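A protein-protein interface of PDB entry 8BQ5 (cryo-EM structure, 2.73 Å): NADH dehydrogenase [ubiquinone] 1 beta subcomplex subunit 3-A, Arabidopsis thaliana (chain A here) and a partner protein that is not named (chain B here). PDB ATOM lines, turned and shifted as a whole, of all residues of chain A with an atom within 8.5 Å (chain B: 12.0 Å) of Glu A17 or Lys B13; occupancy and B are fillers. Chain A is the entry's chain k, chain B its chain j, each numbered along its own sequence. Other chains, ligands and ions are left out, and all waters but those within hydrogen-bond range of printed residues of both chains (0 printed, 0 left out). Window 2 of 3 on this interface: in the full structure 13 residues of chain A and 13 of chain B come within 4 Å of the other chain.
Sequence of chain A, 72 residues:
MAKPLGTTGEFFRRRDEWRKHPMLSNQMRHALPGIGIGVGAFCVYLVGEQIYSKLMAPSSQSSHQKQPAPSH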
ATOM      1  N   GLU A  10     -23.957  -6.907   3.156  1.00  0.00           N
ATOM      2  CA  GLU A  10     -22.732  -7.734   3.361  1.00  0.00           C
ATOM      3  C   GLU A  10     -21.912  -7.772   2.067  1.00  0.00           C
ATOM      4  O   GLU A  10     -20.680  -7.813   2.163  1.00  0.00           O
ATOM      5  CB  GLU A  10     -23.104  -9.140   3.837  1.00  0.00           C
ATOM      6  CG  GLU A  10     -21.930  -9.976   4.328  1.00  0.00           C
ATOM      7  CD  GLU A  10     -20.943  -9.307   5.274  1.00  0.00           C
ATOM      8  OE1 GLU A  10     -21.378  -8.798   6.324  1.00  0.00           O
ATOM      9  OE2 GLU A  10     -19.736  -9.317   4.965  1.00  0.00           O
ATOM     10  N   PHE A  11     -22.568  -7.747   0.908  1.00  0.00           N
ATOM     11  CA  PHE A  11     -21.822  -7.711  -0.377  1.00  0.00           C
ATOM     12  C   PHE A  11     -20.862  -6.526  -0.374  1.00  0.00           C
ATOM     13  O   PHE A  11     -19.670  -6.723  -0.659  1.00  0.00           O
ATOM     14  CB  PHE A  11     -22.775  -7.605  -1.564  1.00  0.00           C
ATOM     15  CG  PHE A  11     -22.082  -7.348  -2.877  1.00  0.00           C
ATOM     16  CD1 PHE A  11     -21.013  -8.132  -3.282  1.00  0.00           C
ATOM     17  CD2 PHE A  11     -22.491  -6.316  -3.702  1.00  0.00           C
ATOM     18  CE1 PHE A  11     -20.373  -7.900  -4.487  1.00  0.00           C
ATOM     19  CE2 PHE A  11     -21.848  -6.084  -4.906  1.00  0.00           C
ATOM     20  CZ  PHE A  11     -20.791  -6.872  -5.294  1.00  0.00           C
ATOM     21  N   PHE A  12     -21.371  -5.338  -0.050  1.00  0.00           N
ATOM     22  CA  PHE A  12     -20.527  -4.115  -0.088  1.00  0.00           C
ATOM     23  C   PHE A  12     -19.505  -4.162   1.047  1.00  0.00           C
ATOM     24  O   PHE A  12     -18.394  -3.663   0.837  1.00  0.00           O
ATOM     25  CB  PHE A  12     -21.409  -2.868  -0.095  1.00  0.00           C
ATOM     26  CG  PHE A  12     -22.045  -2.624  -1.442  1.00  0.00           C
ATOM     27  CD1 PHE A  12     -21.260  -2.432  -2.567  1.00  0.00           C
ATOM     28  CD2 PHE A  12     -23.421  -2.621  -1.594  1.00  0.00           C
ATOM     29  CE1 PHE A  12     -21.837  -2.221  -3.810  1.00  0.00           C
ATOM     30  CE2 PHE A  12     -23.998  -2.413  -2.839  1.00  0.00           C
ATOM     31  CZ  PHE A  12     -23.205  -2.217  -3.944  1.00  0.00           C
ATOM     32  N   ARG A  13     -19.847  -4.787   2.175  1.00  0.00           N
ATOM     33  CA  ARG A  13     -18.852  -4.945   3.265  1.00  0.00           C
ATOM     34  C   ARG A  13     -17.686  -5.789   2.744  1.00  0.00           C
ATOM     35  O   ARG A  13     -16.533  -5.459   3.079  1.00  0.00           O
ATOM     36  CB  ARG A  13     -19.517  -5.547   4.504  1.00  0.00           C
ATOM     37  CG  ARG A  13     -18.553  -5.713   5.669  1.00  0.00           C
ATOM     38  CD  ARG A  13     -19.217  -6.241   6.921  1.00  0.00           C
ATOM     39  NE  ARG A  13     -18.301  -6.379   8.044  1.00  0.00           N
ATOM     40  CZ  ARG A  13     -18.679  -6.637   9.288  1.00  0.00           C
ATOM     41  NH1 ARG A  13     -19.962  -6.782   9.575  1.00  0.00           N
ATOM     42  NH2 ARG A  13     -17.775  -6.747  10.244  1.00  0.00           N
ATOM     43  N   ARG A  14     -17.974  -6.819   1.945  1.00  0.00           N
ATOM     44  CA  ARG A  14     -16.904  -7.661   1.341  1.00  0.00           C
ATOM     45  C   ARG A  14     -16.067  -6.837   0.355  1.00  0.00           C
ATOM     46  O   ARG A  14     -14.843  -7.065   0.305  1.00  0.00           O
ATOM     47  CB  ARG A  14     -17.526  -8.891   0.676  1.00  0.00           C
ATOM     48  CG  ARG A  14     -18.059  -9.921   1.660  1.00  0.00           C
ATOM     49  CD  ARG A  14     -18.701 -11.094   0.947  1.00  0.00           C
ATOM     50  NE  ARG A  14     -19.947 -11.521   1.564  1.00  0.00           N
ATOM     51  CZ  ARG A  14     -20.210 -12.762   1.958  1.00  0.00           C
ATOM     52  NH1 ARG A  14     -19.311 -13.719   1.800  1.00  0.00           N
ATOM     53  NH2 ARG A  14     -21.374 -13.045   2.512  1.00  0.00           N
ATOM     54  N   ARG A  15     -16.695  -5.941  -0.412  1.00  0.00           N
ATOM     55  CA  ARG A  15     -15.975  -5.123  -1.380  1.00  0.00           C
ATOM     56  C   ARG A  15     -15.051  -4.111  -0.716  1.00  0.00           C
ATOM     57  O   ARG A  15     -14.024  -3.753  -1.302  1.00  0.00           O
ATOM     58  CB  ARG A  15     -16.964  -4.406  -2.301  1.00  0.00           C
ATOM     59  CG  ARG A  15     -17.808  -5.345  -3.148  1.00  0.00           C
ATOM     60  CD  ARG A  15     -16.916  -6.254  -3.971  1.00  0.00           C
ATOM     61  NE  ARG A  15     -15.834  -5.519  -4.614  1.00  0.00           N
ATOM     62  CZ  ARG A  15     -14.740  -6.081  -5.106  1.00  0.00           C
ATOM     63  NH1 ARG A  15     -14.525  -7.382  -5.002  1.00  0.00           N
ATOM     64  NH2 ARG A  15     -13.831  -5.318  -5.706  1.00  0.00           N
ATOM     65  N   ASP A  16     -15.379  -3.655   0.491  1.00  0.00           N
ATOM     66  CA  ASP A  16     -14.602  -2.637   1.183  1.00  0.00           C
ATOM     67  C   ASP A  16     -13.552  -3.226   2.120  1.00  0.00           C
ATOM     68  O   ASP A  16     -13.227  -2.602   3.137  1.00  0.00           O
ATOM     69  CB  ASP A  16     -15.530  -1.707   1.968  1.00  0.00           C
ATOM     70  CG  ASP A  16     -16.569  -1.039   1.091  1.00  0.00           C
ATOM     71  OD1 ASP A  16     -16.249  -0.690  -0.064  1.00  0.00           O
ATOM     72  OD2 ASP A  16     -17.709  -0.857   1.560  1.00  0.00           O
ATOM     73  N   GLU A  17     -13.020  -4.411   1.810  1.00  0.00           N
ATOM     74  CA  GLU A  17     -12.019  -5.011   2.686  1.00  0.00           C
ATOM     75  C   GLU A  17     -10.690  -4.273   2.614  1.00  0.00           C
ATOM     76  O   GLU A  17      -9.933  -4.262   3.591  1.00  0.00           O
ATOM     77  CB  GLU A  17     -11.828  -6.486   2.340  1.00  0.00           C
ATOM     78  CG  GLU A  17     -11.975  -7.401   3.539  1.00  0.00           C
ATOM     79  CD  GLU A  17     -13.377  -7.372   4.108  1.00  0.00           C
ATOM     80  OE1 GLU A  17     -14.295  -7.906   3.452  1.00  0.00           O
ATOM     81  OE2 GLU A  17     -13.566  -6.798   5.201  1.00  0.00           O
ATOM     82  N   TRP A  18     -10.387  -3.655   1.471  1.00  0.00           N
ATOM     83  CA  TRP A  18      -9.141  -2.913   1.323  1.00  0.00           C
ATOM     84  C   TRP A  18      -9.087  -1.680   2.212  1.00  0.00           C
ATOM     85  O   TRP A  18      -7.996  -1.165   2.475  1.00  0.00           O
ATOM     86  CB  TRP A  18      -8.946  -2.515  -0.140  1.00  0.00           C
ATOM     87  CG  TRP A  18      -9.957  -1.522  -0.645  1.00  0.00           C
ATOM     88  CD1 TRP A  18     -11.134  -1.804  -1.272  1.00  0.00           C
ATOM     89  CD2 TRP A  18      -9.867  -0.091  -0.589  1.00  0.00           C
ATOM     90  NE1 TRP A  18     -11.789  -0.643  -1.599  1.00  0.00           N
ATOM     91  CE2 TRP A  18     -11.032   0.423  -1.191  1.00  0.00           C
ATOM     92  CE3 TRP A  18      -8.920   0.803  -0.083  1.00  0.00           C
ATOM     93  CZ2 TRP A  18     -11.274   1.788  -1.304  1.00  0.00           C
ATOM     94  CZ3 TRP A  18      -9.162   2.158  -0.196  1.00  0.00           C
ATOM     95  CH2 TRP A  18     -10.329   2.638  -0.801  1.00  0.00           C
ATOM     96  N   ARG A  19     -10.238  -1.203   2.687  1.00  0.00           N
ATOM     97  CA  ARG A  19     -10.287   0.008   3.494  1.00  0.00           C
ATOM     98  C   ARG A  19      -9.676  -0.175   4.877  1.00  0.00           C
ATOM     99  O   ARG A  19      -9.527   0.813   5.603  1.00  0.00           O
ATOM    100  CB  ARG A  19     -11.732   0.486   3.622  1.00  0.00           C
ATOM    101  CG  ARG A  19     -12.224   1.262   2.410  1.00  0.00           C
ATOM    102  CD  ARG A  19     -13.733   1.384   2.408  1.00  0.00           C
ATOM    103  NE  ARG A  19     -14.280   1.463   1.060  1.00  0.00           N
ATOM    104  CZ  ARG A  19     -14.419   2.594   0.382  1.00  0.00           C
ATOM    105  NH1 ARG A  19     -14.012   3.750   0.878  1.00  0.00           N
ATOM    106  NH2 ARG A  19     -14.979   2.564  -0.823  1.00  0.00           N
ATOM    107  N   LYS A  20      -9.333  -1.405   5.262  1.00  0.00           N
ATOM    108  CA  LYS A  20      -8.711  -1.680   6.550  1.00  0.00           C
ATOM    109  C   LYS A  20      -7.196  -1.509   6.522  1.00  0.00           C
ATOM    110  O   LYS A  20      -6.503  -2.074   7.379  1.00  0.00           O
ATOM    111  CB  LYS A  20      -9.070  -3.094   7.015  1.00  0.00           C
ATOM    112  CG  LYS A  20     -10.567  -3.370   7.073  1.00  0.00           C
ATOM    113  CD  LYS A  20     -11.315  -2.240   7.767  1.00  0.00           C
ATOM    114  CE  LYS A  20     -12.751  -2.631   8.080  1.00  0.00           C
ATOM    115  NZ  LYS A  20     -13.128  -2.275   9.479  1.00  0.00           N
ATOM    116  N   HIS A  21      -6.688  -0.742   5.564  1.00  0.00           N
ATOM    117  CA  HIS A  21      -5.254  -0.571   5.397  1.00  0.00           C
ATOM    118  C   HIS A  21      -4.635  -0.026   6.682  1.00  0.00           C
ATOM    119  O   HIS A  21      -5.212   0.870   7.313  1.00  0.00           O
ATOM    120  CB  HIS A  21      -4.976   0.384   4.233  1.00  0.00           C
ATOM    121  CG  HIS A  21      -3.758   0.041   3.437  1.00  0.00           C
ATOM    122  ND1 HIS A  21      -2.482   0.142   3.947  1.00  0.00           N
ATOM    123  CD2 HIS A  21      -3.619  -0.371   2.156  1.00  0.00           C
ATOM    124  CE1 HIS A  21      -1.611  -0.218   3.022  1.00  0.00           C
ATOM    125  NE2 HIS A  21      -2.275  -0.531   1.924  1.00  0.00           N
ATOM    126  N   PRO A  22      -3.477  -0.545   7.104  1.00  0.00           N
ATOM    127  CA  PRO A  22      -2.847  -0.033   8.334  1.00  0.00           C
ATOM    128  C   PRO A  22      -2.684   1.476   8.362  1.00  0.00           C
ATOM    129  O   PRO A  22      -3.024   2.109   9.369  1.00  0.00           O
ATOM    130  CB  PRO A  22      -1.490  -0.746   8.343  1.00  0.00           C
ATOM    131  CG  PRO A  22      -1.741  -2.018   7.620  1.00  0.00           C
ATOM    132  CD  PRO A  22      -2.765  -1.715   6.562  1.00  0.00           C
ATOM    133  N   GLY B   9       6.171   1.821  -1.097  1.00  0.00           N
ATOM    134  CA  GLY B   9       4.750   1.727  -0.811  1.00  0.00           C
ATOM    135  C   GLY B   9       4.326   0.365  -0.296  1.00  0.00           C
ATOM    136  O   GLY B   9       4.990  -0.638  -0.553  1.00  0.00           O
ATOM    137  N   ILE B  10       3.208   0.330   0.428  1.00  0.00           N
ATOM    138  CA  ILE B  10       2.702  -0.886   1.054  1.00  0.00           C
ATOM    139  C   ILE B  10       1.378  -1.255   0.400  1.00  0.00           C
ATOM    140  O   ILE B  10       0.442  -0.447   0.376  1.00  0.00           O
ATOM    141  CB  ILE B  10       2.539  -0.707   2.574  1.00  0.00           C
ATOM    142  CG1 ILE B  10       3.811  -0.105   3.173  1.00  0.00           C
ATOM    143  CG2 ILE B  10       2.235  -2.036   3.234  1.00  0.00           C
ATOM    144  CD1 ILE B  10       3.654   0.358   4.600  1.00  0.00           C
ATOM    145  N   THR B  11       1.297  -2.481  -0.113  1.00  0.00           N
ATOM    146  CA  THR B  11       0.150  -2.957  -0.879  1.00  0.00           C
ATOM    147  C   THR B  11      -0.734  -3.816   0.016  1.00  0.00           C
ATOM    148  O   THR B  11      -0.227  -4.589   0.837  1.00  0.00           O
ATOM    149  CB  THR B  11       0.612  -3.753  -2.102  1.00  0.00           C
ATOM    150  OG1 THR B  11       1.442  -2.923  -2.926  1.00  0.00           O
ATOM    151  CG2 THR B  11      -0.580  -4.224  -2.923  1.00  0.00           C
ATOM    152  N   TYR B  12      -2.050  -3.682  -0.146  1.00  0.00           N
ATOM    153  CA  TYR B  12      -3.032  -4.421   0.642  1.00  0.00           C
ATOM    154  C   TYR B  12      -4.230  -4.689  -0.261  1.00  0.00           C
ATOM    155  O   TYR B  12      -5.099  -3.826  -0.417  1.00  0.00           O
ATOM    156  CB  TYR B  12      -3.423  -3.622   1.891  1.00  0.00           C
ATOM    157  CG  TYR B  12      -4.509  -4.192   2.792  1.00  0.00           C
ATOM    158  CD1 TYR B  12      -4.261  -5.232   3.671  1.00  0.00           C
ATOM    159  CD2 TYR B  12      -5.799  -3.680   2.744  1.00  0.00           C
ATOM    160  CE1 TYR B  12      -5.252  -5.735   4.473  1.00  0.00           C
ATOM    161  CE2 TYR B  12      -6.802  -4.187   3.547  1.00  0.00           C
ATOM    162  CZ  TYR B  12      -6.518  -5.221   4.409  1.00  0.00           C
ATOM    163  OH  TYR B  12      -7.498  -5.743   5.219  1.00  0.00           O
ATOM    164  N   LYS B  13      -4.276  -5.889  -0.834  1.00  0.00           N
ATOM    165  CA  LYS B  13      -5.324  -6.319  -1.762  1.00  0.00           C
ATOM    166  C   LYS B  13      -5.612  -5.255  -2.819  1.00  0.00           C
ATOM    167  O   LYS B  13      -6.703  -4.690  -2.904  1.00  0.00           O
ATOM    168  CB  LYS B  13      -6.603  -6.719  -1.028  1.00  0.00           C
ATOM    169  CG  LYS B  13      -6.547  -8.121  -0.436  1.00  0.00           C
ATOM    170  CD  LYS B  13      -7.861  -8.548   0.209  1.00  0.00           C
ATOM    171  CE  LYS B  13      -8.042  -7.980   1.605  1.00  0.00           C
ATOM    172  NZ  LYS B  13      -8.356  -6.526   1.597  1.00  0.00           N
ATOM    173  N   GLY B  14      -4.596  -4.987  -3.632  1.00  0.00           N
ATOM    174  CA  GLY B  14      -4.778  -4.157  -4.805  1.00  0.00           C
ATOM    175  C   GLY B  14      -4.457  -2.694  -4.601  1.00  0.00           C
ATOM    176  O   GLY B  14      -3.832  -2.069  -5.462  1.00  0.00           O
ATOM    177  N   VAL B  15      -4.872  -2.133  -3.471  1.00  0.00           N
ATOM    178  CA  VAL B  15      -4.635  -0.720  -3.205  1.00  0.00           C
ATOM    179  C   VAL B  15      -3.220  -0.540  -2.675  1.00  0.00           C
ATOM    180  O   VAL B  15      -2.747  -1.312  -1.831  1.00  0.00           O
ATOM    181  CB  VAL B  15      -5.696  -0.155  -2.243  1.00  0.00           C
ATOM    182  CG1 VAL B  15      -7.070  -0.657  -2.647  1.00  0.00           C
ATOM    183  CG2 VAL B  15      -5.408  -0.531  -0.800  1.00  0.00           C
ATOM    184  N   THR B  16      -2.517   0.445  -3.221  1.00  0.00           N
ATOM    185  CA  THR B  16      -1.162   0.777  -2.816  1.00  0.00           C
ATOM    186  C   THR B  16      -1.139   2.223  -2.349  1.00  0.00           C
ATOM    187  O   THR B  16      -1.629   3.112  -3.051  1.00  0.00           O
ATOM    188  CB  THR B  16      -0.178   0.578  -3.973  1.00  0.00           C
ATOM    189  OG1 THR B  16      -0.207  -0.788  -4.406  1.00  0.00           O
ATOM    190  CG2 THR B  16       1.234   0.937  -3.543  1.00  0.00           C
ATOM    191  N   VAL B  17      -0.589   2.456  -1.162  1.00  0.00           N
ATOM    192  CA  VAL B  17      -0.412   3.800  -0.626  1.00  0.00           C
ATOM    193  C   VAL B  17       1.075   4.025  -0.398  1.00  0.00           C
ATOM    194  O   VAL B  17       1.690   3.365   0.449  1.00  0.00           O
ATOM    195  CB  VAL B  17      -1.226   4.009   0.664  1.00  0.00           C
ATOM    196  CG1 VAL B  17      -1.120   2.799   1.572  1.00  0.00           C
ATOM    197  CG2 VAL B  17      -0.772   5.272   1.385  1.00  0.00           C
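The side-chain hydroxyl of Tyr B12 sits close to the backbone carbonyl oxygen of Glu A17, 3.3 Å away.
NZ of Lys B13 lies close to O of Glu A17 (3.4 Å).
A ring nitrogen (NE2) of His A21 sits at hydrogen-bond distance from the backbone carbonyl oxygen (O) of Ile B10, at 3.1 Å.
The backbone NH of Ile B10 sits at hydrogen-bond distance from the backbone carbonyl oxygen of Val B17, 3.4 Å away.
Among the printed residues, merely in contact across the chains: His A21 with Tyr B12, Trp A18 with Tyr B12, His A21 with Val B17, His A21 with Val B15, Trp A18 with Val B15, Trp A18 with Lys B13 and Lys A20 with Tyr B12.
Of the printed residues of chain A, Lys B13 touches Glu A17 (3.4 Å) and Trp A18 (3.5 Å).
No residue of chain B comes within 4 Å of Arg A13.
No residue of chain B comes within 4 Å of Arg A15.
Of chain B, only Tyr B12 (3.6 Å) comes within 4 Å of Lys A20.
His A21 touches just these residues of chain B: Ile B10, Tyr B12, Val B15 and Val B17.
Printed residues of chain A within 4 Å of Ile B10: His A21.
Of the printed residues of chain A, Val B15 touches Trp A18 (3.5 Å) and His A21 (3.5 Å).
Of the printed residues of chain A, Val B17 touches His A21.
Printed residues of chain A within 4 Å of Tyr B12: Glu A17, Trp A18, Lys A20 and His A21.
The nearest residue of chain A that does not touch Lys B13 is Arg A19 (5.8 Å).
Printed residues of chain B that touch a printed residue of chain A: Ile B10, Tyr B12, Lys B13, Val B15 and Val B17.
Hydrophobic or aromatic side chains of chain B within 4 Å of the printed part of chain A: Tyr B12, Val B15 and Val B17.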
